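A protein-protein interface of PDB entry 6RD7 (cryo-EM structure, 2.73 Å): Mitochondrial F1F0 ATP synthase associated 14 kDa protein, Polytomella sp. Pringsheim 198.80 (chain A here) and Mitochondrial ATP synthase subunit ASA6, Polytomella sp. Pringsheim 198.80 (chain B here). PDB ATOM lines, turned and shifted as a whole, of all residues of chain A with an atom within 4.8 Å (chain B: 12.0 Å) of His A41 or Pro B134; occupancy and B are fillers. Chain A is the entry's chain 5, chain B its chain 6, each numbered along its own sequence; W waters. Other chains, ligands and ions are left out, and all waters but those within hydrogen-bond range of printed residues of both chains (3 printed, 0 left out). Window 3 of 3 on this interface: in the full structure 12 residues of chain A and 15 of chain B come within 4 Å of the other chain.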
ATOM      1  N   GLU A  37      10.283 -20.878 -12.083  1.00  0.00           N
ATOM      2  CA  GLU A  37       9.989 -19.651 -11.355  1.00  0.00           C
ATOM      3  C   GLU A  37       8.578 -19.147 -11.640  1.00  0.00           C
ATOM      4  O   GLU A  37       7.900 -18.647 -10.739  1.00  0.00           O
ATOM      5  CB  GLU A  37      11.036 -18.609 -11.726  1.00  0.00           C
ATOM      6  CG  GLU A  37      10.833 -17.251 -11.150  1.00  0.00           C
ATOM      7  CD  GLU A  37      12.011 -16.365 -11.430  1.00  0.00           C
ATOM      8  OE1 GLU A  37      13.116 -16.902 -11.647  1.00  0.00           O
ATOM      9  OE2 GLU A  37      11.830 -15.134 -11.457  1.00  0.00           O
ATOM     10  N   HIS A  38       8.101 -19.306 -12.869  1.00  0.00           N
ATOM     11  CA  HIS A  38       6.764 -18.855 -13.223  1.00  0.00           C
ATOM     12  C   HIS A  38       5.702 -19.785 -12.670  1.00  0.00           C
ATOM     13  O   HIS A  38       4.680 -19.329 -12.155  1.00  0.00           O
ATOM     14  CB  HIS A  38       6.631 -18.757 -14.743  1.00  0.00           C
ATOM     15  CG  HIS A  38       5.218 -18.628 -15.216  1.00  0.00           C
ATOM     16  ND1 HIS A  38       4.513 -17.448 -15.138  1.00  0.00           N
ATOM     17  CD2 HIS A  38       4.377 -19.533 -15.768  1.00  0.00           C
ATOM     18  CE1 HIS A  38       3.300 -17.630 -15.621  1.00  0.00           C
ATOM     19  NE2 HIS A  38       3.190 -18.887 -16.010  1.00  0.00           N
ATOM     20  N   LYS A  39       5.927 -21.094 -12.755  1.00  0.00           N
ATOM     21  CA  LYS A  39       4.861 -22.035 -12.475  1.00  0.00           C
ATOM     22  C   LYS A  39       4.741 -22.327 -10.994  1.00  0.00           C
ATOM     23  O   LYS A  39       3.688 -22.778 -10.553  1.00  0.00           O
ATOM     24  CB  LYS A  39       5.073 -23.320 -13.262  1.00  0.00           C
ATOM     25  CG  LYS A  39       4.541 -23.243 -14.662  1.00  0.00           C
ATOM     26  CD  LYS A  39       4.898 -24.471 -15.432  1.00  0.00           C
ATOM     27  CE  LYS A  39       4.405 -24.387 -16.847  1.00  0.00           C
ATOM     28  NZ  LYS A  39       5.066 -25.439 -17.637  1.00  0.00           N
ATOM     29  N   LEU A  40       5.781 -22.046 -10.200  1.00  0.00           N
ATOM     30  CA  LEU A  40       5.584 -22.064  -8.752  1.00  0.00           C
ATOM     31  C   LEU A  40       4.570 -21.006  -8.336  1.00  0.00           C
ATOM     32  O   LEU A  40       3.593 -21.301  -7.632  1.00  0.00           O
ATOM     33  CB  LEU A  40       6.917 -21.857  -8.031  1.00  0.00           C
ATOM     34  CG  LEU A  40       6.956 -22.020  -6.507  1.00  0.00           C
ATOM     35  CD1 LEU A  40       8.255 -22.615  -6.123  1.00  0.00           C
ATOM     36  CD2 LEU A  40       6.815 -20.705  -5.756  1.00  0.00           C
ATOM     37  N   HIS A  41       4.778 -19.774  -8.800  1.00  0.00           N
ATOM     38  CA  HIS A  41       3.867 -18.674  -8.521  1.00  0.00           C
ATOM     39  C   HIS A  41       2.490 -18.919  -9.123  1.00  0.00           C
ATOM     40  O   HIS A  41       1.471 -18.665  -8.475  1.00  0.00           O
ATOM     41  CB  HIS A  41       4.474 -17.380  -9.053  1.00  0.00           C
ATOM     42  CG  HIS A  41       3.694 -16.153  -8.710  1.00  0.00           C
ATOM     43  ND1 HIS A  41       2.599 -15.740  -9.434  1.00  0.00           N
ATOM     44  CD2 HIS A  41       3.869 -15.236  -7.732  1.00  0.00           C
ATOM     45  CE1 HIS A  41       2.123 -14.628  -8.908  1.00  0.00           C
ATOM     46  NE2 HIS A  41       2.877 -14.299  -7.876  1.00  0.00           N
ATOM     47  N   ALA A  42       2.440 -19.449 -10.346  1.00  0.00           N
ATOM     48  CA  ALA A  42       1.167 -19.662 -11.021  1.00  0.00           C
ATOM     49  C   ALA A  42       0.380 -20.798 -10.388  1.00  0.00           C
ATOM     50  O   ALA A  42      -0.843 -20.707 -10.260  1.00  0.00           O
ATOM     51  CB  ALA A  42       1.401 -19.936 -12.503  1.00  0.00           C
ATOM     52  N   CYS A  43       1.061 -21.863  -9.960  1.00  0.00           N
ATOM     53  CA  CYS A  43       0.376 -22.977  -9.325  1.00  0.00           C
ATOM     54  C   CYS A  43      -0.115 -22.600  -7.940  1.00  0.00           C
ATOM     55  O   CYS A  43      -1.213 -23.001  -7.544  1.00  0.00           O
ATOM     56  CB  CYS A  43       1.299 -24.187  -9.258  1.00  0.00           C
ATOM     57  SG  CYS A  43       1.472 -25.036 -10.823  1.00  0.00           S
ATOM     58  N   TRP A  44       0.658 -21.796  -7.204  1.00  0.00           N
ATOM     59  CA  TRP A  44       0.179 -21.336  -5.906  1.00  0.00           C
ATOM     60  C   TRP A  44      -0.990 -20.371  -6.054  1.00  0.00           C
ATOM     61  O   TRP A  44      -1.953 -20.437  -5.283  1.00  0.00           O
ATOM     62  CB  TRP A  44       1.315 -20.692  -5.120  1.00  0.00           C
ATOM     63  CG  TRP A  44       2.080 -21.648  -4.258  1.00  0.00           C
ATOM     64  CD1 TRP A  44       3.396 -21.966  -4.369  1.00  0.00           C
ATOM     65  CD2 TRP A  44       1.579 -22.402  -3.148  1.00  0.00           C
ATOM     66  NE1 TRP A  44       3.749 -22.871  -3.404  1.00  0.00           N
ATOM     67  CE2 TRP A  44       2.650 -23.155  -2.641  1.00  0.00           C
ATOM     68  CE3 TRP A  44       0.327 -22.518  -2.535  1.00  0.00           C
ATOM     69  CZ2 TRP A  44       2.511 -24.005  -1.554  1.00  0.00           C
ATOM     70  CZ3 TRP A  44       0.192 -23.360  -1.461  1.00  0.00           C
ATOM     71  CH2 TRP A  44       1.277 -24.093  -0.979  1.00  0.00           C
ATOM     72  N   ALA A  45      -0.948 -19.498  -7.064  1.00  0.00           N
ATOM     73  CA  ALA A  45      -2.047 -18.565  -7.283  1.00  0.00           C
ATOM     74  C   ALA A  45      -3.300 -19.280  -7.770  1.00  0.00           C
ATOM     75  O   ALA A  45      -4.418 -18.878  -7.432  1.00  0.00           O
ATOM     76  CB  ALA A  45      -1.627 -17.490  -8.280  1.00  0.00           C
ATOM     77  N   TYR B 126      14.094  -1.423 -14.008  1.00  0.00           N
ATOM     78  CA  TYR B 126      14.115  -2.646 -13.207  1.00  0.00           C
ATOM     79  C   TYR B 126      12.717  -3.028 -12.734  1.00  0.00           C
ATOM     80  O   TYR B 126      12.311  -4.192 -12.841  1.00  0.00           O
ATOM     81  CB  TYR B 126      15.051  -2.467 -12.008  1.00  0.00           C
ATOM     82  CG  TYR B 126      15.037  -3.622 -11.030  1.00  0.00           C
ATOM     83  CD1 TYR B 126      15.733  -4.789 -11.303  1.00  0.00           C
ATOM     84  CD2 TYR B 126      14.331  -3.545  -9.835  1.00  0.00           C
ATOM     85  CE1 TYR B 126      15.720  -5.847 -10.426  1.00  0.00           C
ATOM     86  CE2 TYR B 126      14.306  -4.602  -8.955  1.00  0.00           C
ATOM     87  CZ  TYR B 126      15.006  -5.749  -9.255  1.00  0.00           C
ATOM     88  OH  TYR B 126      14.999  -6.806  -8.380  1.00  0.00           O
ATOM     89  N   PHE B 127      11.956  -2.057 -12.236  1.00  0.00           N
ATOM     90  CA  PHE B 127      10.631  -2.380 -11.722  1.00  0.00           C
ATOM     91  C   PHE B 127       9.625  -2.583 -12.848  1.00  0.00           C
ATOM     92  O   PHE B 127       8.585  -3.216 -12.646  1.00  0.00           O
ATOM     93  CB  PHE B 127      10.170  -1.296 -10.756  1.00  0.00           C
ATOM     94  CG  PHE B 127      10.700  -1.475  -9.373  1.00  0.00           C
ATOM     95  CD1 PHE B 127      10.156  -2.425  -8.531  1.00  0.00           C
ATOM     96  CD2 PHE B 127      11.758  -0.711  -8.917  1.00  0.00           C
ATOM     97  CE1 PHE B 127      10.647  -2.599  -7.258  1.00  0.00           C
ATOM     98  CE2 PHE B 127      12.252  -0.880  -7.644  1.00  0.00           C
ATOM     99  CZ  PHE B 127      11.696  -1.826  -6.815  1.00  0.00           C
ATOM    100  N   ALA B 128       9.916  -2.066 -14.043  1.00  0.00           N
ATOM    101  CA  ALA B 128       9.070  -2.358 -15.192  1.00  0.00           C
ATOM    102  C   ALA B 128       9.345  -3.750 -15.724  1.00  0.00           C
ATOM    103  O   ALA B 128       8.443  -4.418 -16.239  1.00  0.00           O
ATOM    104  CB  ALA B 128       9.289  -1.317 -16.287  1.00  0.00           C
ATOM    105  N   PHE B 129      10.593  -4.205 -15.619  1.00  0.00           N
ATOM    106  CA  PHE B 129      10.901  -5.573 -16.013  1.00  0.00           C
ATOM    107  C   PHE B 129      10.351  -6.560 -14.995  1.00  0.00           C
ATOM    108  O   PHE B 129       9.989  -7.684 -15.352  1.00  0.00           O
ATOM    109  CB  PHE B 129      12.409  -5.755 -16.186  1.00  0.00           C
ATOM    110  CG  PHE B 129      12.946  -5.260 -17.506  1.00  0.00           C
ATOM    111  CD1 PHE B 129      12.151  -4.552 -18.391  1.00  0.00           C
ATOM    112  CD2 PHE B 129      14.257  -5.506 -17.858  1.00  0.00           C
ATOM    113  CE1 PHE B 129      12.653  -4.102 -19.591  1.00  0.00           C
ATOM    114  CE2 PHE B 129      14.766  -5.058 -19.057  1.00  0.00           C
ATOM    115  CZ  PHE B 129      13.962  -4.357 -19.923  1.00  0.00           C
ATOM    116  N   ARG B 130      10.254  -6.143 -13.729  1.00  0.00           N
ATOM    117  CA  ARG B 130       9.629  -6.984 -12.711  1.00  0.00           C
ATOM    118  C   ARG B 130       8.139  -7.176 -12.962  1.00  0.00           C
ATOM    119  O   ARG B 130       7.565  -8.179 -12.531  1.00  0.00           O
ATOM    120  CB  ARG B 130       9.846  -6.382 -11.325  1.00  0.00           C
ATOM    121  CG  ARG B 130      11.090  -6.868 -10.626  1.00  0.00           C
ATOM    122  CD  ARG B 130      11.153  -6.358  -9.202  1.00  0.00           C
ATOM    123  NE  ARG B 130      10.425  -7.214  -8.273  1.00  0.00           N
ATOM    124  CZ  ARG B 130      10.927  -8.306  -7.709  1.00  0.00           C
ATOM    125  NH1 ARG B 130      10.188  -9.020  -6.876  1.00  0.00           N
ATOM    126  NH2 ARG B 130      12.165  -8.686  -7.977  1.00  0.00           N
ATOM    127  N   GLY B 131       7.496  -6.234 -13.644  1.00  0.00           N
ATOM    128  CA  GLY B 131       6.101  -6.381 -13.998  1.00  0.00           C
ATOM    129  C   GLY B 131       5.827  -7.194 -15.238  1.00  0.00           C
ATOM    130  O   GLY B 131       4.669  -7.507 -15.517  1.00  0.00           O
ATOM    131  N   MET B 132       6.862  -7.547 -15.999  1.00  0.00           N
ATOM    132  CA  MET B 132       6.669  -8.359 -17.194  1.00  0.00           C
ATOM    133  C   MET B 132       6.439  -9.818 -16.835  1.00  0.00           C
ATOM    134  O   MET B 132       5.646 -10.508 -17.481  1.00  0.00           O
ATOM    135  CB  MET B 132       7.874  -8.225 -18.121  1.00  0.00           C
ATOM    136  CG  MET B 132       8.009  -6.868 -18.757  1.00  0.00           C
ATOM    137  SD  MET B 132       9.587  -6.676 -19.586  1.00  0.00           S
ATOM    138  CE  MET B 132       9.505  -8.008 -20.765  1.00  0.00           C
ATOM    139  N   ALA B 133       7.124 -10.298 -15.830  1.00  0.00           N
ATOM    140  CA  ALA B 133       6.928 -11.658 -15.356  1.00  0.00           C
ATOM    141  C   ALA B 133       5.830 -11.678 -14.307  1.00  0.00           C
ATOM    142  O   ALA B 133       5.851 -10.854 -13.389  1.00  0.00           O
ATOM    143  CB  ALA B 133       8.211 -12.214 -14.767  1.00  0.00           C
ATOM    144  N   PRO B 134       4.853 -12.582 -14.411  1.00  0.00           N
ATOM    145  CA  PRO B 134       3.810 -12.648 -13.376  1.00  0.00           C
ATOM    146  C   PRO B 134       4.308 -13.151 -12.034  1.00  0.00           C
ATOM    147  O   PRO B 134       3.639 -12.924 -11.022  1.00  0.00           O
ATOM    148  CB  PRO B 134       2.777 -13.603 -13.987  1.00  0.00           C
ATOM    149  CG  PRO B 134       3.029 -13.554 -15.438  1.00  0.00           C
ATOM    150  CD  PRO B 134       4.500 -13.389 -15.587  1.00  0.00           C
ATOM    151  N   ALA B 135       5.464 -13.819 -11.989  1.00  0.00           N
ATOM    152  CA  ALA B 135       5.997 -14.302 -10.721  1.00  0.00           C
ATOM    153  C   ALA B 135       6.510 -13.167  -9.848  1.00  0.00           C
ATOM    154  O   ALA B 135       6.538 -13.296  -8.622  1.00  0.00           O
ATOM    155  CB  ALA B 135       7.112 -15.313 -10.967  1.00  0.00           C
ATOM    156  N   THR B 136       6.925 -12.058 -10.451  1.00  0.00           N
ATOM    157  CA  THR B 136       7.408 -10.917  -9.698  1.00  0.00           C
ATOM    158  C   THR B 136       6.474  -9.723  -9.753  1.00  0.00           C
ATOM    159  O   THR B 136       6.713  -8.741  -9.048  1.00  0.00           O
ATOM    160  CB  THR B 136       8.793 -10.494 -10.201  1.00  0.00           C
ATOM    161  OG1 THR B 136       8.775 -10.413 -11.627  1.00  0.00           O
ATOM    162  CG2 THR B 136       9.818 -11.507  -9.786  1.00  0.00           C
ATOM    163  N   ALA B 137       5.422  -9.783 -10.567  1.00  0.00           N
ATOM    164  CA  ALA B 137       4.468  -8.686 -10.621  1.00  0.00           C
ATOM    165  C   ALA B 137       3.592  -8.659  -9.378  1.00  0.00           C
ATOM    166  O   ALA B 137       3.137  -7.591  -8.955  1.00  0.00           O
ATOM    167  CB  ALA B 137       3.612  -8.799 -11.880  1.00  0.00           C
ATOM    168  N   SER B 138       3.348  -9.820  -8.779  1.00  0.00           N
ATOM    169  CA  SER B 138       2.502  -9.934  -7.604  1.00  0.00           C
ATOM    170  C   SER B 138       3.284 -10.563  -6.465  1.00  0.00           C
ATOM    171  O   SER B 138       4.331 -11.181  -6.665  1.00  0.00           O
ATOM    172  CB  SER B 138       1.253 -10.775  -7.891  1.00  0.00           C
ATOM    173  OG  SER B 138       0.444 -10.173  -8.881  1.00  0.00           O
ATOM    174  N   THR B 139       2.758 -10.391  -5.258  1.00  0.00           N
ATOM    175  CA  THR B 139       3.218 -11.167  -4.120  1.00  0.00           C
ATOM    176  C   THR B 139       2.717 -12.600  -4.265  1.00  0.00           C
ATOM    177  O   THR B 139       1.602 -12.840  -4.734  1.00  0.00           O
ATOM    178  CB  THR B 139       2.714 -10.534  -2.817  1.00  0.00           C
ATOM    179  OG1 THR B 139       3.143  -9.168  -2.759  1.00  0.00           O
ATOM    180  CG2 THR B 139       3.245 -11.256  -1.582  1.00  0.00           C
ATOM    181  N   LEU B 140       3.573 -13.559  -3.904  1.00  0.00           N
ATOM    182  CA  LEU B 140       3.203 -14.966  -3.915  1.00  0.00           C
ATOM    183  C   LEU B 140       2.081 -15.239  -2.926  1.00  0.00           C
ATOM    184  O   LEU B 140       2.291 -15.206  -1.711  1.00  0.00           O
ATOM    185  CB  LEU B 140       4.411 -15.839  -3.586  1.00  0.00           C
ATOM    186  CG  LEU B 140       4.133 -17.333  -3.500  1.00  0.00           C
ATOM    187  CD1 LEU B 140       3.844 -17.904  -4.862  1.00  0.00           C
ATOM    188  CD2 LEU B 140       5.303 -18.023  -2.888  1.00  0.00           C
ATOM    189  N   ASN B 141       0.884 -15.488  -3.443  1.00  0.00           N
ATOM    190  CA  ASN B 141      -0.293 -15.746  -2.631  1.00  0.00           C
ATOM    191  C   ASN B 141      -0.603 -17.232  -2.668  1.00  0.00           C
ATOM    192  O   ASN B 141      -0.867 -17.791  -3.735  1.00  0.00           O
ATOM    193  CB  ASN B 141      -1.491 -14.940  -3.127  1.00  0.00           C
ATOM    194  CG  ASN B 141      -2.658 -14.997  -2.175  1.00  0.00           C
ATOM    195  OD1 ASN B 141      -3.447 -15.939  -2.196  1.00  0.00           O
ATOM    196  ND2 ASN B 141      -2.769 -13.989  -1.319  1.00  0.00           N
ATOM    197  N   GLY B 142      -0.550 -17.866  -1.508  1.00  0.00           N
ATOM    198  CA  GLY B 142      -0.702 -19.298  -1.414  1.00  0.00           C
ATOM    199  C   GLY B 142      -1.365 -19.738  -0.133  1.00  0.00           C
ATOM    200  O   GLY B 142      -2.501 -19.363   0.164  1.00  0.00           O
ATOM    201  N   LEU B 143      -0.661 -20.616   0.577  1.00  0.00           N
ATOM    202  CA  LEU B 143      -1.052 -21.082   1.900  1.00  0.00           C
ATOM    203  C   LEU B 143      -1.295 -19.928   2.868  1.00  0.00           C
ATOM    204  O   LEU B 143      -0.430 -19.079   3.084  1.00  0.00           O
ATOM    205  CB  LEU B 143       0.043 -21.995   2.440  1.00  0.00           C
ATOM    206  CG  LEU B 143      -0.002 -22.398   3.904  1.00  0.00           C
ATOM    207  CD1 LEU B 143      -1.209 -23.216   4.106  1.00  0.00           C
ATOM    208  CD2 LEU B 143       1.226 -23.190   4.279  1.00  0.00           C
ATOM    209  N   LYS B 144      -2.491 -19.900   3.443  1.00  0.00           N
ATOM    210  CA  LYS B 144      -2.846 -18.953   4.485  1.00  0.00           C
ATOM    211  C   LYS B 144      -2.575 -19.579   5.843  1.00  0.00           C
ATOM    212  O   LYS B 144      -2.478 -20.800   5.971  1.00  0.00           O
ATOM    213  CB  LYS B 144      -4.315 -18.543   4.393  1.00  0.00           C
ATOM    214  CG  LYS B 144      -4.675 -17.781   3.143  1.00  0.00           C
ATOM    215  CD  LYS B 144      -3.843 -16.530   3.005  1.00  0.00           C
ATOM    216  CE  LYS B 144      -4.086 -15.873   1.666  1.00  0.00           C
ATOM    217  NZ  LYS B 144      -4.072 -16.869   0.562  1.00  0.00           N
HETATM  218  O   HOH W   1       6.673 -15.506 -14.249  1.00  0.00           O
HETATM  219  O   HOH W   2       0.950 -16.855  -6.204  1.00  0.00           O
HETATM  220  O   HOH W   3      -0.214 -14.254  -6.807  1.00  0.00           O
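O of Gly B142 lies within hydrogen-bond range of NZ of Lys B144. The side-chain amino group (NZ) of Lys B144 sits at hydrogen-bond distance from the side-chain amide oxygen (OD1) of Asn B141 (3.0 Å).
Printed residues of chain B that touch a printed residue of chain A: Pro B134, Ala B135, Ser B138, Thr B139, Leu B140, Asn B141, Gly B142 and Leu B143. Hydrophobic or aromatic side chains of chain B that line the printed part of chain A: Ala B135 and Leu B140. Printed residues of chain A that touch a printed residue of chain B: Glu A37, His A41, Trp A44 and Ala A45. Among the printed residues, no Asp or Glu carboxylate lies within 4 Å of a Lys or Arg side-chain nitrogen of the other chain.
Glu A37 touches Ala B135. Ala B135 touches His A41 (O to CD2, 3.4 Å). O of Ser B138 touches NE2 of His A41, at 3.6 Å. His A41 touches Thr B139 (NE2 to O, 3.7 Å). CA of His A41 touches CD1 of Leu B140, at 3.7 Å. Trp A44 touches Leu B140. CE3 of Trp A44 touches CA of Gly B142 (3.6 Å). Leu B143 touches Trp A44 (N to CZ3, 3.5 Å). Ala A45 touches Asn B141.
Printed residues of chain B within 4 Å of Glu A37: Ala B135. No residue of chain B comes within 4 Å of His A38. No residue of chain B comes within 4 Å of Leu A40. His A41 touches just these residues of chain B: Pro B134 (3.1 Å), Ala B135 (3.4 Å), Ser B138 (3.6 Å), Thr B139 (3.7 Å) and Leu B140 (3.7 Å). No residue of chain B comes within 4 Å of Cys A43. Of chain B, only Asn B141 comes within 4 Å of Ala A45. Of the printed residues of chain A, Thr B139 touches His A41 (3.7 Å). Of the printed residues of chain A, Leu B140 touches His A41 (3.7 Å) and Trp A44 (3.8 Å). Of the printed residues of chain A, Leu B143 touches Trp A44 (3.5 Å). The nearest printed residue of chain A that does not touch Leu B143 is Ala A45 (7.7 Å).
Water W2 lies within hydrogen-bond range of the backbone carbonyl oxygen of His A41 (3.0 Å), the backbone NH of Asn B141 (3.1 Å) and the backbone NH of Ala A45 (3.4 Å). Water W1 bridges ND1 of His A38 (3.0 Å) and N of Ala B135 (3.1 Å). Water W3 lies within hydrogen-bond range of the backbone carbonyl oxygen (O) of Thr B139 (3.1 Å) and a ring nitrogen (NE2) of His A41 (3.3 Å).
The backbone carbonyl oxygen (O) of Trp A44 lies close to the backbone carbonyl oxygen (O) of Asn B141 (3.3 Å). ND1 of His A41 sits close to O of Pro B134 (3.4 Å).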
